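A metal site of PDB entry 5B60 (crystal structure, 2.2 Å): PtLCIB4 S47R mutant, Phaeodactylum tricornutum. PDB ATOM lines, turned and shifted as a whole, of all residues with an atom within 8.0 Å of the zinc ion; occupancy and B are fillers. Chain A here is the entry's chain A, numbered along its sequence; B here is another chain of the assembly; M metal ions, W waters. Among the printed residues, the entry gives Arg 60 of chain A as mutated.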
ATOM      1  N   LEU A  58      -7.738  10.225 -20.271  1.00  0.00           N
ATOM      2  CA  LEU A  58      -8.267  11.508 -19.830  1.00  0.00           C
ATOM      3  C   LEU A  58      -9.570  11.199 -19.126  1.00  0.00           C
ATOM      4  O   LEU A  58     -10.135  10.114 -19.312  1.00  0.00           O
ATOM      5  CB  LEU A  58      -8.504  12.473 -21.024  1.00  0.00           C
ATOM      6  CG  LEU A  58      -7.333  12.641 -22.019  1.00  0.00           C
ATOM      7  CD1 LEU A  58      -7.765  13.320 -23.321  1.00  0.00           C
ATOM      8  CD2 LEU A  58      -6.181  13.385 -21.377  1.00  0.00           C
ATOM      9  N   CYS A  59     -10.033  12.147 -18.314  1.00  0.00           N
ATOM     10  CA  CYS A  59     -11.332  12.047 -17.671  1.00  0.00           C
ATOM     11  C   CYS A  59     -12.379  11.970 -18.750  1.00  0.00           C
ATOM     12  O   CYS A  59     -12.196  12.526 -19.857  1.00  0.00           O
ATOM     13  CB  CYS A  59     -11.622  13.237 -16.763  1.00  0.00           C
ATOM     14  SG  CYS A  59     -13.248  13.140 -15.947  1.00  0.00           S
ATOM     15  N   ARG A  60     -13.480  11.311 -18.398  1.00  0.00           N
ATOM     16  CA  ARG A  60     -14.505  10.941 -19.361  1.00  0.00           C
ATOM     17  C   ARG A  60     -15.645  11.949 -19.433  1.00  0.00           C
ATOM     18  O   ARG A  60     -16.614  11.752 -20.158  1.00  0.00           O
ATOM     19  CB  ARG A  60     -15.040   9.568 -19.019  1.00  0.00           C
ATOM     20  CG  ARG A  60     -13.921   8.592 -18.818  1.00  0.00           C
ATOM     21  CD  ARG A  60     -13.394   8.176 -20.156  1.00  0.00           C
ATOM     22  NE  ARG A  60     -14.304   7.196 -20.727  1.00  0.00           N
ATOM     23  CZ  ARG A  60     -14.299   5.916 -20.397  1.00  0.00           C
ATOM     24  NH1 ARG A  60     -13.415   5.447 -19.514  1.00  0.00           N
ATOM     25  NH2 ARG A  60     -15.153   5.069 -20.955  1.00  0.00           N
ATOM     26  N   ASP A  61     -15.523  13.026 -18.649  1.00  0.00           N
ATOM     27  CA  ASP A  61     -16.393  14.177 -18.839  1.00  0.00           C
ATOM     28  C   ASP A  61     -16.230  14.632 -20.283  1.00  0.00           C
ATOM     29  O   ASP A  61     -15.120  14.595 -20.817  1.00  0.00           O
ATOM     30  CB  ASP A  61     -16.012  15.290 -17.867  1.00  0.00           C
ATOM     31  CG  ASP A  61     -17.101  16.322 -17.695  1.00  0.00           C
ATOM     32  OD1 ASP A  61     -17.280  17.165 -18.586  1.00  0.00           O
ATOM     33  OD2 ASP A  61     -17.774  16.279 -16.642  1.00  0.00           O
ATOM     34  N   GLU A  62     -17.321  15.032 -20.948  1.00  0.00           N
ATOM     35  CA  GLU A  62     -17.257  15.467 -22.353  1.00  0.00           C
ATOM     36  C   GLU A  62     -16.421  16.697 -22.665  1.00  0.00           C
ATOM     37  O   GLU A  62     -16.099  16.937 -23.787  1.00  0.00           O
ATOM     38  CB  GLU A  62     -18.650  15.637 -22.977  1.00  0.00           C
ATOM     39  CG  GLU A  62     -18.618  16.201 -24.399  1.00  0.00           C
ATOM     40  CD  GLU A  62     -19.935  16.128 -25.164  1.00  0.00           C
ATOM     41  OE1 GLU A  62     -21.017  16.286 -24.595  1.00  0.00           O
ATOM     42  OE2 GLU A  62     -19.876  15.926 -26.391  1.00  0.00           O
ATOM     43  N   VAL A  63     -16.064  17.481 -21.679  1.00  0.00           N
ATOM     44  CA  VAL A  63     -15.253  18.657 -21.964  1.00  0.00           C
ATOM     45  C   VAL A  63     -13.835  18.280 -22.416  1.00  0.00           C
ATOM     46  O   VAL A  63     -13.137  19.092 -23.013  1.00  0.00           O
ATOM     47  CB  VAL A  63     -15.150  19.624 -20.746  1.00  0.00           C
ATOM     48  CG1 VAL A  63     -16.519  19.985 -20.242  1.00  0.00           C
ATOM     49  CG2 VAL A  63     -14.322  18.994 -19.632  1.00  0.00           C
ATOM     50  N   THR A  64     -13.420  17.039 -22.140  1.00  0.00           N
ATOM     51  CA  THR A  64     -12.073  16.590 -22.468  1.00  0.00           C
ATOM     52  C   THR A  64     -11.927  16.123 -23.918  1.00  0.00           C
ATOM     53  O   THR A  64     -10.817  15.897 -24.386  1.00  0.00           O
ATOM     54  CB  THR A  64     -11.595  15.428 -21.560  1.00  0.00           C
ATOM     55  OG1 THR A  64     -12.343  14.247 -21.858  1.00  0.00           O
ATOM     56  CG2 THR A  64     -11.748  15.760 -20.078  1.00  0.00           C
ATOM     57  N   GLY A  83     -10.119   6.518 -17.100  1.00  0.00           N
ATOM     58  CA  GLY A  83     -11.206   6.356 -16.157  1.00  0.00           C
ATOM     59  C   GLY A  83     -11.509   7.685 -15.498  1.00  0.00           C
ATOM     60  O   GLY A  83     -11.214   8.748 -16.056  1.00  0.00           O
ATOM     61  N   LEU A  84     -12.086   7.622 -14.307  1.00  0.00           N
ATOM     62  CA  LEU A  84     -12.438   8.824 -13.576  1.00  0.00           C
ATOM     63  C   LEU A  84     -11.191   9.673 -13.337  1.00  0.00           C
ATOM     64  O   LEU A  84     -10.117   9.142 -13.019  1.00  0.00           O
ATOM     65  CB  LEU A  84     -13.129   8.455 -12.266  1.00  0.00           C
ATOM     66  CG  LEU A  84     -14.537   7.888 -12.468  1.00  0.00           C
ATOM     67  CD1 LEU A  84     -15.151   7.441 -11.172  1.00  0.00           C
ATOM     68  CD2 LEU A  84     -15.455   8.882 -13.146  1.00  0.00           C
ATOM     69  N   ALA A  85     -11.349  10.975 -13.512  1.00  0.00           N
ATOM     70  CA  ALA A  85     -10.297  11.971 -13.294  1.00  0.00           C
ATOM     71  C   ALA A  85      -9.129  11.883 -14.287  1.00  0.00           C
ATOM     72  O   ALA A  85      -8.233  12.724 -14.256  1.00  0.00           O
ATOM     73  CB  ALA A  85      -9.767  11.882 -11.859  1.00  0.00           C
ATOM     74  N   GLY A  86      -9.135  10.887 -15.188  1.00  0.00           N
ATOM     75  CA  GLY A  86      -8.038  10.682 -16.123  1.00  0.00           C
ATOM     76  C   GLY A  86      -7.129   9.524 -15.718  1.00  0.00           C
ATOM     77  O   GLY A  86      -6.156   9.222 -16.404  1.00  0.00           O
ATOM     78  N   SER A 114      -4.516  15.055 -16.165  1.00  0.00           N
ATOM     79  CA  SER A 114      -5.605  15.518 -15.317  1.00  0.00           C
ATOM     80  C   SER A 114      -6.259  16.599 -16.100  1.00  0.00           C
ATOM     81  O   SER A 114      -5.713  17.037 -17.092  1.00  0.00           O
ATOM     82  CB  SER A 114      -5.099  16.061 -13.984  1.00  0.00           C
ATOM     83  OG  SER A 114      -4.419  17.287 -14.192  1.00  0.00           O
ATOM     84  N   HIS A 115      -7.432  17.043 -15.670  1.00  0.00           N
ATOM     85  CA  HIS A 115      -7.967  18.234 -16.306  1.00  0.00           C
ATOM     86  C   HIS A 115      -8.672  19.131 -15.308  1.00  0.00           C
ATOM     87  O   HIS A 115      -8.926  18.733 -14.172  1.00  0.00           O
ATOM     88  CB  HIS A 115      -8.881  17.885 -17.468  1.00  0.00           C
ATOM     89  CG  HIS A 115     -10.251  17.450 -17.050  1.00  0.00           C
ATOM     90  ND1 HIS A 115     -11.395  18.077 -17.498  1.00  0.00           N
ATOM     91  CD2 HIS A 115     -10.676  16.420 -16.285  1.00  0.00           C
ATOM     92  CE1 HIS A 115     -12.456  17.482 -16.993  1.00  0.00           C
ATOM     93  NE2 HIS A 115     -12.041  16.452 -16.268  1.00  0.00           N
ATOM     94  N   VAL A 116      -8.973  20.346 -15.767  1.00  0.00           N
ATOM     95  CA  VAL A 116      -9.472  21.410 -14.923  1.00  0.00           C
ATOM     96  C   VAL A 116     -10.145  22.462 -15.775  1.00  0.00           C
ATOM     97  O   VAL A 116      -9.644  22.835 -16.836  1.00  0.00           O
ATOM     98  CB  VAL A 116      -8.342  22.050 -14.088  1.00  0.00           C
ATOM     99  CG1 VAL A 116      -7.298  22.686 -14.980  1.00  0.00           C
ATOM    100  CG2 VAL A 116      -8.913  23.063 -13.082  1.00  0.00           C
ATOM    101  N   GLY A 117     -11.299  22.926 -15.320  1.00  0.00           N
ATOM    102  CA  GLY A 117     -12.013  23.985 -16.017  1.00  0.00           C
ATOM    103  C   GLY A 117     -11.534  25.342 -15.562  1.00  0.00           C
ATOM    104  O   GLY A 117     -11.063  25.494 -14.434  1.00  0.00           O
ATOM    105  N   ALA A 137     -18.688  21.928 -11.529  1.00  0.00           N
ATOM    106  CA  ALA A 137     -17.315  21.596 -11.177  1.00  0.00           C
ATOM    107  C   ALA A 137     -16.604  20.753 -12.254  1.00  0.00           C
ATOM    108  O   ALA A 137     -17.188  19.831 -12.840  1.00  0.00           O
ATOM    109  CB  ALA A 137     -17.280  20.863  -9.849  1.00  0.00           C
ATOM    110  N   CYS A 138     -15.340  21.095 -12.486  1.00  0.00           N
ATOM    111  CA  CYS A 138     -14.513  20.458 -13.523  1.00  0.00           C
ATOM    112  C   CYS A 138     -13.042  20.619 -13.111  1.00  0.00           C
ATOM    113  O   CYS A 138     -12.525  21.746 -13.106  1.00  0.00           O
ATOM    114  CB  CYS A 138     -14.810  21.092 -14.889  1.00  0.00           C
ATOM    115  SG  CYS A 138     -13.670  20.776 -16.248  1.00  0.00           S
ATOM    116  N   CYS A 139     -12.382  19.535 -12.723  1.00  0.00           N
ATOM    117  CA  CYS A 139     -12.890  18.151 -12.769  1.00  0.00           C
ATOM    118  C   CYS A 139     -13.815  17.782 -11.607  1.00  0.00           C
ATOM    119  O   CYS A 139     -13.384  17.797 -10.454  1.00  0.00           O
ATOM    120  CB  CYS A 139     -11.715  17.165 -12.801  1.00  0.00           C
ATOM    121  SG  CYS A 139     -12.131  15.367 -12.961  1.00  0.00           S
ATOM    122  N   GLY A 140     -15.063  17.422 -11.912  1.00  0.00           N
ATOM    123  CA  GLY A 140     -16.027  16.998 -10.900  1.00  0.00           C
ATOM    124  C   GLY A 140     -15.544  15.871 -10.003  1.00  0.00           C
ATOM    125  O   GLY A 140     -15.644  15.968  -8.783  1.00  0.00           O
ATOM    126  N   SER A 141     -15.008  14.814 -10.606  1.00  0.00           N
ATOM    127  CA  SER A 141     -14.560  13.651  -9.854  1.00  0.00           C
ATOM    128  C   SER A 141     -13.329  13.951  -8.994  1.00  0.00           C
ATOM    129  O   SER A 141     -13.256  13.515  -7.841  1.00  0.00           O
ATOM    130  CB  SER A 141     -14.262  12.506 -10.813  1.00  0.00           C
ATOM    131  OG  SER A 141     -13.333  11.589 -10.259  1.00  0.00           O
ATOM    132  N   ALA A 142     -12.365  14.686  -9.536  1.00  0.00           N
ATOM    133  CA  ALA A 142     -11.188  15.062  -8.750  1.00  0.00           C
ATOM    134  C   ALA A 142     -11.569  15.930  -7.541  1.00  0.00           C
ATOM    135  O   ALA A 142     -11.119  15.674  -6.424  1.00  0.00           O
ATOM    136  CB  ALA A 142     -10.190  15.791  -9.595  1.00  0.00           C
ATOM    137  N   VAL A 143     -12.393  16.941  -7.803  1.00  0.00           N
ATOM    138  CA  VAL A 143     -12.873  17.865  -6.784  1.00  0.00           C
ATOM    139  C   VAL A 143     -13.567  17.130  -5.644  1.00  0.00           C
ATOM    140  O   VAL A 143     -13.246  17.325  -4.471  1.00  0.00           O
ATOM    141  CB  VAL A 143     -13.827  18.896  -7.414  1.00  0.00           C
ATOM    142  CG1 VAL A 143     -14.764  19.480  -6.368  1.00  0.00           C
ATOM    143  CG2 VAL A 143     -13.034  19.979  -8.139  1.00  0.00           C
ATOM    144  N   ASN A 247      -9.529  23.115 -19.663  1.00  0.00           N
ATOM    145  CA  ASN A 247     -10.749  23.295 -20.424  1.00  0.00           C
ATOM    146  C   ASN A 247     -11.297  24.718 -20.263  1.00  0.00           C
ATOM    147  O   ASN A 247     -11.558  25.190 -19.145  1.00  0.00           O
ATOM    148  CB  ASN A 247     -11.756  22.210 -19.999  1.00  0.00           C
ATOM    149  CG  ASN A 247     -11.195  20.799 -20.210  1.00  0.00           C
ATOM    150  OD1 ASN A 247     -11.090  20.015 -19.279  1.00  0.00           O
ATOM    151  ND2 ASN A 247     -10.796  20.491 -21.454  1.00  0.00           N
ATOM    152  N   ALA B  97     -20.952  10.991 -15.701  1.00  0.00           N
ATOM    153  CA  ALA B  97     -20.173  11.491 -16.833  1.00  0.00           C
ATOM    154  C   ALA B  97     -20.923  11.228 -18.128  1.00  0.00           C
ATOM    155  O   ALA B  97     -21.095  12.140 -18.935  1.00  0.00           O
ATOM    156  CB  ALA B  97     -18.813  10.844 -16.856  1.00  0.00           C
HETATM  157 ZN    ZN M   1     -13.184  15.308 -14.943  1.00  0.00          ZN
HETATM  158  O   HOH W   1     -15.077  16.468 -15.202  1.00  0.00           O
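Water W1 lies within hydrogen-bond range of the side-chain carboxylate (OD2) of Asp 61 (3.1 Å) and the backbone NH (N) of Gly 140 (3.4 Å).
SG of Cys 138 lies close to ND1 of His 115. OD1 of Asn 247 lies within hydrogen-bond range of ND1 of His 115 (2.6 Å). The side-chain sulfur (SG) of Cys 139 sits close to the backbone NH (N) of Ser 141 (3.8 Å). The side-chain sulfur (SG) of Cys 139 sits close to the backbone NH (N) of Ala 142, 3.5 Å away. SG of Cys 59 lies close to N of Asp 61, at 3.5 Å. The side-chain sulfur (SG) of Cys 59 sits close to the backbone NH (N) of Ala 85. The backbone carbonyl oxygen (O) of Cys 59 sits at hydrogen-bond distance from the side-chain hydroxyl (OG1) of Thr 64, 2.6 Å away.
The zinc ion is bound by a ring nitrogen (NE2) of His 115, water W1, the side-chain sulfur (SG) of Cys 139 and the side-chain sulfur (SG) of Cys 59. The zinc ion has four donor atoms within binding distance.
Within 4 Å of the zinc ion: Cys 59, His 115 and Cys 139.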
